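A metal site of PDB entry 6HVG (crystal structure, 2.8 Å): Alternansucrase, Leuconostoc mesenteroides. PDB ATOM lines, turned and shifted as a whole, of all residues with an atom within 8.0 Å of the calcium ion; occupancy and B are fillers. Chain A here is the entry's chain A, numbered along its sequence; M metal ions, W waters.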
ATOM      1  N   LYS A 554      -3.978 -23.363   0.021  1.00  0.00           N
ATOM      2  CA  LYS A 554      -4.433 -24.676  -0.463  1.00  0.00           C
ATOM      3  C   LYS A 554      -5.943 -24.702  -0.438  1.00  0.00           C
ATOM      4  O   LYS A 554      -6.558 -24.575   0.623  1.00  0.00           O
ATOM      5  CB  LYS A 554      -3.919 -25.814   0.404  1.00  0.00           C
ATOM      6  CG  LYS A 554      -2.402 -25.882   0.458  1.00  0.00           C
ATOM      7  CD  LYS A 554      -1.935 -26.525   1.737  1.00  0.00           C
ATOM      8  CE  LYS A 554      -0.429 -26.384   1.946  1.00  0.00           C
ATOM      9  NZ  LYS A 554       0.259 -27.556   1.354  1.00  0.00           N
ATOM     10  N   LEU A 555      -6.538 -24.853  -1.618  1.00  0.00           N
ATOM     11  CA  LEU A 555      -7.965 -24.767  -1.761  1.00  0.00           C
ATOM     12  C   LEU A 555      -8.621 -26.131  -1.740  1.00  0.00           C
ATOM     13  O   LEU A 555      -8.049 -27.112  -2.238  1.00  0.00           O
ATOM     14  CB  LEU A 555      -8.268 -24.091  -3.065  1.00  0.00           C
ATOM     15  CG  LEU A 555      -7.664 -22.688  -3.268  1.00  0.00           C
ATOM     16  CD1 LEU A 555      -8.126 -22.063  -4.588  1.00  0.00           C
ATOM     17  CD2 LEU A 555      -7.972 -21.744  -2.137  1.00  0.00           C
ATOM     18  N   GLY A 556      -9.790 -26.219  -1.114  1.00  0.00           N
ATOM     19  CA  GLY A 556     -10.621 -27.425  -1.198  1.00  0.00           C
ATOM     20  C   GLY A 556     -10.118 -28.573  -0.358  1.00  0.00           C
ATOM     21  O   GLY A 556     -10.339 -29.726  -0.705  1.00  0.00           O
ATOM     22  N   GLY A 573     -12.789 -29.806  -2.567  1.00  0.00           N
ATOM     23  CA  GLY A 573     -13.785 -29.035  -1.839  1.00  0.00           C
ATOM     24  C   GLY A 573     -14.121 -27.720  -2.502  1.00  0.00           C
ATOM     25  O   GLY A 573     -13.264 -27.100  -3.138  1.00  0.00           O
ATOM     26  N   SER A 574     -15.365 -27.289  -2.332  1.00  0.00           N
ATOM     27  CA  SER A 574     -15.805 -25.992  -2.770  1.00  0.00           C
ATOM     28  C   SER A 574     -15.368 -24.994  -1.711  1.00  0.00           C
ATOM     29  O   SER A 574     -16.117 -24.732  -0.792  1.00  0.00           O
ATOM     30  CB  SER A 574     -17.326 -25.986  -2.914  1.00  0.00           C
ATOM     31  OG  SER A 574     -17.755 -27.132  -3.655  1.00  0.00           O
ATOM     32  N   GLU A 575     -14.156 -24.473  -1.856  1.00  0.00           N
ATOM     33  CA  GLU A 575     -13.543 -23.588  -0.887  1.00  0.00           C
ATOM     34  C   GLU A 575     -14.250 -22.264  -0.813  1.00  0.00           C
ATOM     35  O   GLU A 575     -14.298 -21.621   0.245  1.00  0.00           O
ATOM     36  CB  GLU A 575     -12.083 -23.367  -1.254  1.00  0.00           C
ATOM     37  CG  GLU A 575     -11.253 -22.549  -0.248  1.00  0.00           C
ATOM     38  CD  GLU A 575     -11.147 -23.159   1.140  1.00  0.00           C
ATOM     39  OE1 GLU A 575     -10.428 -24.185   1.305  1.00  0.00           O
ATOM     40  OE2 GLU A 575     -11.803 -22.589   2.054  1.00  0.00           O
ATOM     41  N   PHE A 576     -14.828 -21.849  -1.933  1.00  0.00           N
ATOM     42  CA  PHE A 576     -15.461 -20.531  -1.993  1.00  0.00           C
ATOM     43  C   PHE A 576     -16.943 -20.647  -1.820  1.00  0.00           C
ATOM     44  O   PHE A 576     -17.570 -21.439  -2.487  1.00  0.00           O
ATOM     45  CB  PHE A 576     -15.154 -19.856  -3.322  1.00  0.00           C
ATOM     46  CG  PHE A 576     -13.691 -19.589  -3.517  1.00  0.00           C
ATOM     47  CD1 PHE A 576     -13.134 -18.440  -3.038  1.00  0.00           C
ATOM     48  CD2 PHE A 576     -12.906 -20.524  -4.111  1.00  0.00           C
ATOM     49  CE1 PHE A 576     -11.774 -18.203  -3.185  1.00  0.00           C
ATOM     50  CE2 PHE A 576     -11.561 -20.306  -4.276  1.00  0.00           C
ATOM     51  CZ  PHE A 576     -10.990 -19.142  -3.806  1.00  0.00           C
ATOM     52  N   LEU A 577     -17.460 -19.862  -0.878  1.00  0.00           N
ATOM     53  CA  LEU A 577     -18.855 -19.930  -0.511  1.00  0.00           C
ATOM     54  C   LEU A 577     -19.418 -18.542  -0.537  1.00  0.00           C
ATOM     55  O   LEU A 577     -20.246 -18.225  -1.393  1.00  0.00           O
ATOM     56  CB  LEU A 577     -18.979 -20.580   0.893  1.00  0.00           C
ATOM     57  CG  LEU A 577     -20.361 -20.622   1.572  1.00  0.00           C
ATOM     58  CD1 LEU A 577     -21.365 -21.388   0.742  1.00  0.00           C
ATOM     59  CD2 LEU A 577     -20.179 -21.272   2.931  1.00  0.00           C
ATOM     60  N   LEU A 578     -18.982 -17.683   0.393  1.00  0.00           N
ATOM     61  CA  LEU A 578     -19.527 -16.327   0.507  1.00  0.00           C
ATOM     62  C   LEU A 578     -18.448 -15.369   0.899  1.00  0.00           C
ATOM     63  O   LEU A 578     -17.497 -15.724   1.601  1.00  0.00           O
ATOM     64  CB  LEU A 578     -20.646 -16.256   1.549  1.00  0.00           C
ATOM     65  CG  LEU A 578     -22.003 -16.881   1.169  1.00  0.00           C
ATOM     66  CD1 LEU A 578     -22.822 -17.273   2.391  1.00  0.00           C
ATOM     67  CD2 LEU A 578     -22.829 -15.918   0.340  1.00  0.00           C
ATOM     68  N   ASN A 580     -15.547 -12.781   1.728  1.00  0.00           N
ATOM     69  CA  ASN A 580     -14.111 -12.941   1.673  1.00  0.00           C
ATOM     70  C   ASN A 580     -13.750 -14.257   2.271  1.00  0.00           C
ATOM     71  O   ASN A 580     -13.926 -14.445   3.455  1.00  0.00           O
ATOM     72  CB  ASN A 580     -13.418 -11.843   2.453  1.00  0.00           C
ATOM     73  CG  ASN A 580     -13.596 -10.491   1.822  1.00  0.00           C
ATOM     74  OD1 ASN A 580     -12.900 -10.131   0.865  1.00  0.00           O
ATOM     75  ND2 ASN A 580     -14.515  -9.731   2.345  1.00  0.00           N
ATOM     76  N   ASP A 581     -13.230 -15.173   1.464  1.00  0.00           N
ATOM     77  CA  ASP A 581     -12.929 -16.521   1.942  1.00  0.00           C
ATOM     78  C   ASP A 581     -11.566 -16.511   2.663  1.00  0.00           C
ATOM     79  O   ASP A 581     -10.562 -16.176   2.089  1.00  0.00           O
ATOM     80  CB  ASP A 581     -12.960 -17.509   0.779  1.00  0.00           C
ATOM     81  CG  ASP A 581     -12.758 -18.904   1.200  1.00  0.00           C
ATOM     82  OD1 ASP A 581     -13.705 -19.555   1.668  1.00  0.00           O
ATOM     83  OD2 ASP A 581     -11.615 -19.390   0.996  1.00  0.00           O
ATOM     84  N   ILE A 582     -11.588 -16.863   3.933  1.00  0.00           N
ATOM     85  CA  ILE A 582     -10.406 -16.927   4.780  1.00  0.00           C
ATOM     86  C   ILE A 582      -9.524 -18.148   4.432  1.00  0.00           C
ATOM     87  O   ILE A 582     -10.028 -19.251   4.228  1.00  0.00           O
ATOM     88  CB  ILE A 582     -10.819 -16.956   6.259  1.00  0.00           C
ATOM     89  CG1 ILE A 582     -11.418 -15.594   6.627  1.00  0.00           C
ATOM     90  CG2 ILE A 582      -9.633 -17.300   7.157  1.00  0.00           C
ATOM     91  CD1 ILE A 582     -12.169 -15.583   7.946  1.00  0.00           C
ATOM     92  N   ASP A 583      -8.219 -17.918   4.348  1.00  0.00           N
ATOM     93  CA  ASP A 583      -7.255 -18.978   4.062  1.00  0.00           C
ATOM     94  C   ASP A 583      -6.945 -19.778   5.335  1.00  0.00           C
ATOM     95  O   ASP A 583      -5.933 -19.523   6.023  1.00  0.00           O
ATOM     96  CB  ASP A 583      -5.983 -18.382   3.477  1.00  0.00           C
ATOM     97  CG  ASP A 583      -4.920 -19.419   3.166  1.00  0.00           C
ATOM     98  OD1 ASP A 583      -5.233 -20.634   3.102  1.00  0.00           O
ATOM     99  OD2 ASP A 583      -3.752 -18.994   2.982  1.00  0.00           O
ATOM    100  N   ASN A 584      -7.815 -20.740   5.639  1.00  0.00           N
ATOM    101  CA  ASN A 584      -7.607 -21.649   6.765  1.00  0.00           C
ATOM    102  C   ASN A 584      -6.526 -22.729   6.559  1.00  0.00           C
ATOM    103  O   ASN A 584      -6.266 -23.511   7.453  1.00  0.00           O
ATOM    104  CB  ASN A 584      -8.928 -22.293   7.174  1.00  0.00           C
ATOM    105  CG  ASN A 584      -9.976 -21.265   7.615  1.00  0.00           C
ATOM    106  OD1 ASN A 584      -9.715 -20.396   8.435  1.00  0.00           O
ATOM    107  ND2 ASN A 584     -11.167 -21.355   7.037  1.00  0.00           N
ATOM    108  N   ALA A 622     -19.969 -24.713   7.981  1.00  0.00           N
ATOM    109  CA  ALA A 622     -19.422 -24.805   6.627  1.00  0.00           C
ATOM    110  C   ALA A 622     -18.183 -25.672   6.555  1.00  0.00           C
ATOM    111  O   ALA A 622     -17.162 -25.257   6.011  1.00  0.00           O
ATOM    112  CB  ALA A 622     -19.115 -23.398   6.101  1.00  0.00           C
ATOM    113  N   VAL A 623     -18.281 -26.864   7.110  1.00  0.00           N
ATOM    114  CA  VAL A 623     -17.148 -27.780   7.219  1.00  0.00           C
ATOM    115  C   VAL A 623     -16.507 -28.081   5.862  1.00  0.00           C
ATOM    116  O   VAL A 623     -15.281 -28.091   5.742  1.00  0.00           O
ATOM    117  CB  VAL A 623     -17.596 -29.096   7.892  1.00  0.00           C
ATOM    118  CG1 VAL A 623     -16.525 -30.186   7.804  1.00  0.00           C
ATOM    119  CG2 VAL A 623     -17.943 -28.834   9.355  1.00  0.00           C
ATOM    120  N   ASP A 624     -17.332 -28.329   4.858  1.00  0.00           N
ATOM    121  CA  ASP A 624     -16.835 -28.708   3.552  1.00  0.00           C
ATOM    122  C   ASP A 624     -16.263 -27.550   2.737  1.00  0.00           C
ATOM    123  O   ASP A 624     -15.666 -27.768   1.678  1.00  0.00           O
ATOM    124  CB  ASP A 624     -17.952 -29.417   2.794  1.00  0.00           C
ATOM    125  CG  ASP A 624     -18.326 -30.776   3.424  1.00  0.00           C
ATOM    126  OD1 ASP A 624     -17.503 -31.338   4.190  1.00  0.00           O
ATOM    127  OD2 ASP A 624     -19.443 -31.284   3.137  1.00  0.00           O
ATOM    128  N   ASN A 625     -16.416 -26.325   3.237  1.00  0.00           N
ATOM    129  CA  ASN A 625     -15.936 -25.132   2.546  1.00  0.00           C
ATOM    130  C   ASN A 625     -14.654 -24.518   3.142  1.00  0.00           C
ATOM    131  O   ASN A 625     -14.292 -23.389   2.785  1.00  0.00           O
ATOM    132  CB  ASN A 625     -17.031 -24.080   2.570  1.00  0.00           C
ATOM    133  CG  ASN A 625     -18.370 -24.667   2.283  1.00  0.00           C
ATOM    134  OD1 ASN A 625     -19.057 -25.116   3.202  1.00  0.00           O
ATOM    135  ND2 ASN A 625     -18.793 -24.612   1.028  1.00  0.00           N
ATOM    136  N   VAL A 626     -13.990 -25.255   4.033  1.00  0.00           N
ATOM    137  CA  VAL A 626     -12.775 -24.827   4.714  1.00  0.00           C
ATOM    138  C   VAL A 626     -11.765 -25.980   4.813  1.00  0.00           C
ATOM    139  O   VAL A 626     -12.036 -27.103   4.408  1.00  0.00           O
ATOM    140  CB  VAL A 626     -13.074 -24.312   6.134  1.00  0.00           C
ATOM    141  CG1 VAL A 626     -14.086 -23.180   6.089  1.00  0.00           C
ATOM    142  CG2 VAL A 626     -13.529 -25.439   7.064  1.00  0.00           C
ATOM    143  N   ASP A 627     -10.572 -25.665   5.326  1.00  0.00           N
ATOM    144  CA  ASP A 627      -9.499 -26.657   5.509  1.00  0.00           C
ATOM    145  C   ASP A 627      -9.814 -27.539   6.721  1.00  0.00           C
ATOM    146  O   ASP A 627      -9.982 -27.056   7.842  1.00  0.00           O
ATOM    147  CB  ASP A 627      -8.134 -25.959   5.698  1.00  0.00           C
ATOM    148  CG  ASP A 627      -6.953 -26.923   5.582  1.00  0.00           C
ATOM    149  OD1 ASP A 627      -6.952 -28.000   6.211  1.00  0.00           O
ATOM    150  OD2 ASP A 627      -6.007 -26.588   4.869  1.00  0.00           O
ATOM    151  N   PRO A1158     -15.508 -20.049  10.799  1.00  0.00           N
ATOM    152  CA  PRO A1158     -14.181 -19.716  10.287  1.00  0.00           C
ATOM    153  C   PRO A1158     -14.038 -19.487   8.768  1.00  0.00           C
ATOM    154  O   PRO A1158     -12.982 -19.014   8.348  1.00  0.00           O
ATOM    155  CB  PRO A1158     -13.357 -20.941  10.698  1.00  0.00           C
ATOM    156  CG  PRO A1158     -14.326 -22.058  10.653  1.00  0.00           C
ATOM    157  CD  PRO A1158     -15.614 -21.476  11.140  1.00  0.00           C
ATOM    158  N   ASP A1159     -15.064 -19.812   7.964  1.00  0.00           N
ATOM    159  CA  ASP A1159     -14.919 -19.755   6.501  1.00  0.00           C
ATOM    160  C   ASP A1159     -14.774 -18.340   5.936  1.00  0.00           C
ATOM    161  O   ASP A1159     -14.013 -18.139   4.985  1.00  0.00           O
ATOM    162  CB  ASP A1159     -16.076 -20.456   5.809  1.00  0.00           C
ATOM    163  CG  ASP A1159     -15.949 -20.410   4.270  1.00  0.00           C
ATOM    164  OD1 ASP A1159     -15.000 -20.967   3.705  1.00  0.00           O
ATOM    165  OD2 ASP A1159     -16.792 -19.756   3.627  1.00  0.00           O
ATOM    166  N   GLN A1160     -15.505 -17.356   6.468  1.00  0.00           N
ATOM    167  CA  GLN A1160     -15.496 -16.027   5.841  1.00  0.00           C
ATOM    168  C   GLN A1160     -15.740 -14.862   6.780  1.00  0.00           C
ATOM    169  O   GLN A1160     -16.109 -15.041   7.942  1.00  0.00           O
ATOM    170  CB  GLN A1160     -16.498 -15.970   4.658  1.00  0.00           C
ATOM    171  CG  GLN A1160     -17.971 -15.822   5.012  1.00  0.00           C
ATOM    172  CD  GLN A1160     -18.582 -17.076   5.615  1.00  0.00           C
ATOM    173  OE1 GLN A1160     -18.355 -18.185   5.112  1.00  0.00           O
ATOM    174  NE2 GLN A1160     -19.378 -16.915   6.676  1.00  0.00           N
ATOM    175  N   GLU A1177     -16.580 -22.454  -7.549  1.00  0.00           N
ATOM    176  CA  GLU A1177     -16.561 -22.705  -6.103  1.00  0.00           C
ATOM    177  C   GLU A1177     -15.366 -23.518  -5.620  1.00  0.00           C
ATOM    178  O   GLU A1177     -14.918 -23.327  -4.493  1.00  0.00           O
ATOM    179  CB  GLU A1177     -17.851 -23.379  -5.677  1.00  0.00           C
ATOM    180  CG  GLU A1177     -17.991 -24.809  -6.194  1.00  0.00           C
ATOM    181  CD  GLU A1177     -19.403 -25.305  -6.045  1.00  0.00           C
ATOM    182  OE1 GLU A1177     -20.306 -24.726  -6.679  1.00  0.00           O
ATOM    183  OE2 GLU A1177     -19.597 -26.241  -5.272  1.00  0.00           O
ATOM    184  N   ASN A1249      -8.204 -16.376   0.672  1.00  0.00           N
ATOM    185  CA  ASN A1249      -8.186 -17.123  -0.568  1.00  0.00           C
ATOM    186  C   ASN A1249      -8.790 -16.338  -1.709  1.00  0.00           C
ATOM    187  O   ASN A1249      -8.370 -16.472  -2.854  1.00  0.00           O
ATOM    188  CB  ASN A1249      -8.973 -18.425  -0.425  1.00  0.00           C
ATOM    189  CG  ASN A1249      -8.287 -19.426   0.478  1.00  0.00           C
ATOM    190  OD1 ASN A1249      -7.064 -19.416   0.621  1.00  0.00           O
ATOM    191  ND2 ASN A1249      -9.077 -20.287   1.119  1.00  0.00           N
ATOM    192  N   GLY A1250      -9.764 -15.505  -1.408  1.00  0.00           N
ATOM    193  CA  GLY A1250     -10.387 -14.722  -2.461  1.00  0.00           C
ATOM    194  C   GLY A1250     -11.620 -13.979  -2.005  1.00  0.00           C
ATOM    195  O   GLY A1250     -11.774 -13.687  -0.819  1.00  0.00           O
HETATM  196 CA    CA M   1     -13.436 -21.338   2.231  1.00  0.00          CA
HETATM  197  O   HOH W   1     -12.421 -20.539   4.225  1.00  0.00           O
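Of the 26 residues printed, 4 come within 4 Å of the calcium ion.
Water W1 lies within hydrogen-bond range of O of Ile 582 (2.7 Å), O of Asp 1159 (3.0 Å) and ND2 of Asn 584 (3.2 Å).
The calcium ion is bound by OD1 of Asp 581 (1.9 Å), OE2 of Glu 575 (2.1 Å), OD1 of Asp 1159 (2.2 Å), O of Glu 575 (2.2 Å), O of Asn 625 (2.3 Å) and water W1 (2.4 Å). Slightly farther from the calcium ion lies the side-chain carboxylate (OD2) of Asp 581 (2.9 Å).
ND2 of Asn 1249 lies within hydrogen-bond range of OD2 of Asp 581, 2.7 Å away. The side-chain amide oxygen (OD1) of Asn 625 sits close to the backbone carbonyl oxygen (O) of Ala 622 (3.4 Å). The backbone carbonyl oxygen (O) of Glu 1177 is in hydrogen-bond range of the backbone NH (N) of Glu 575. OD2 of Asp 1159 lies close to OE1 of Gln 1160 (2.7 Å). The side-chain carboxylate (OE1) of Glu 575 lies within hydrogen-bond range of the backbone NH (N) of Gly 556. O of Ser 574 is in hydrogen-bond range of ND2 of Asn 625 (3.2 Å). The backbone carbonyl oxygen (O) of Asp 1159 lies within hydrogen-bond range of the backbone NH (N) of Ile 582, at 2.9 Å. The backbone NH (N) of Asp 581 lies within hydrogen-bond range of the backbone carbonyl oxygen (O) of Gly 1250, 3.1 Å away.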
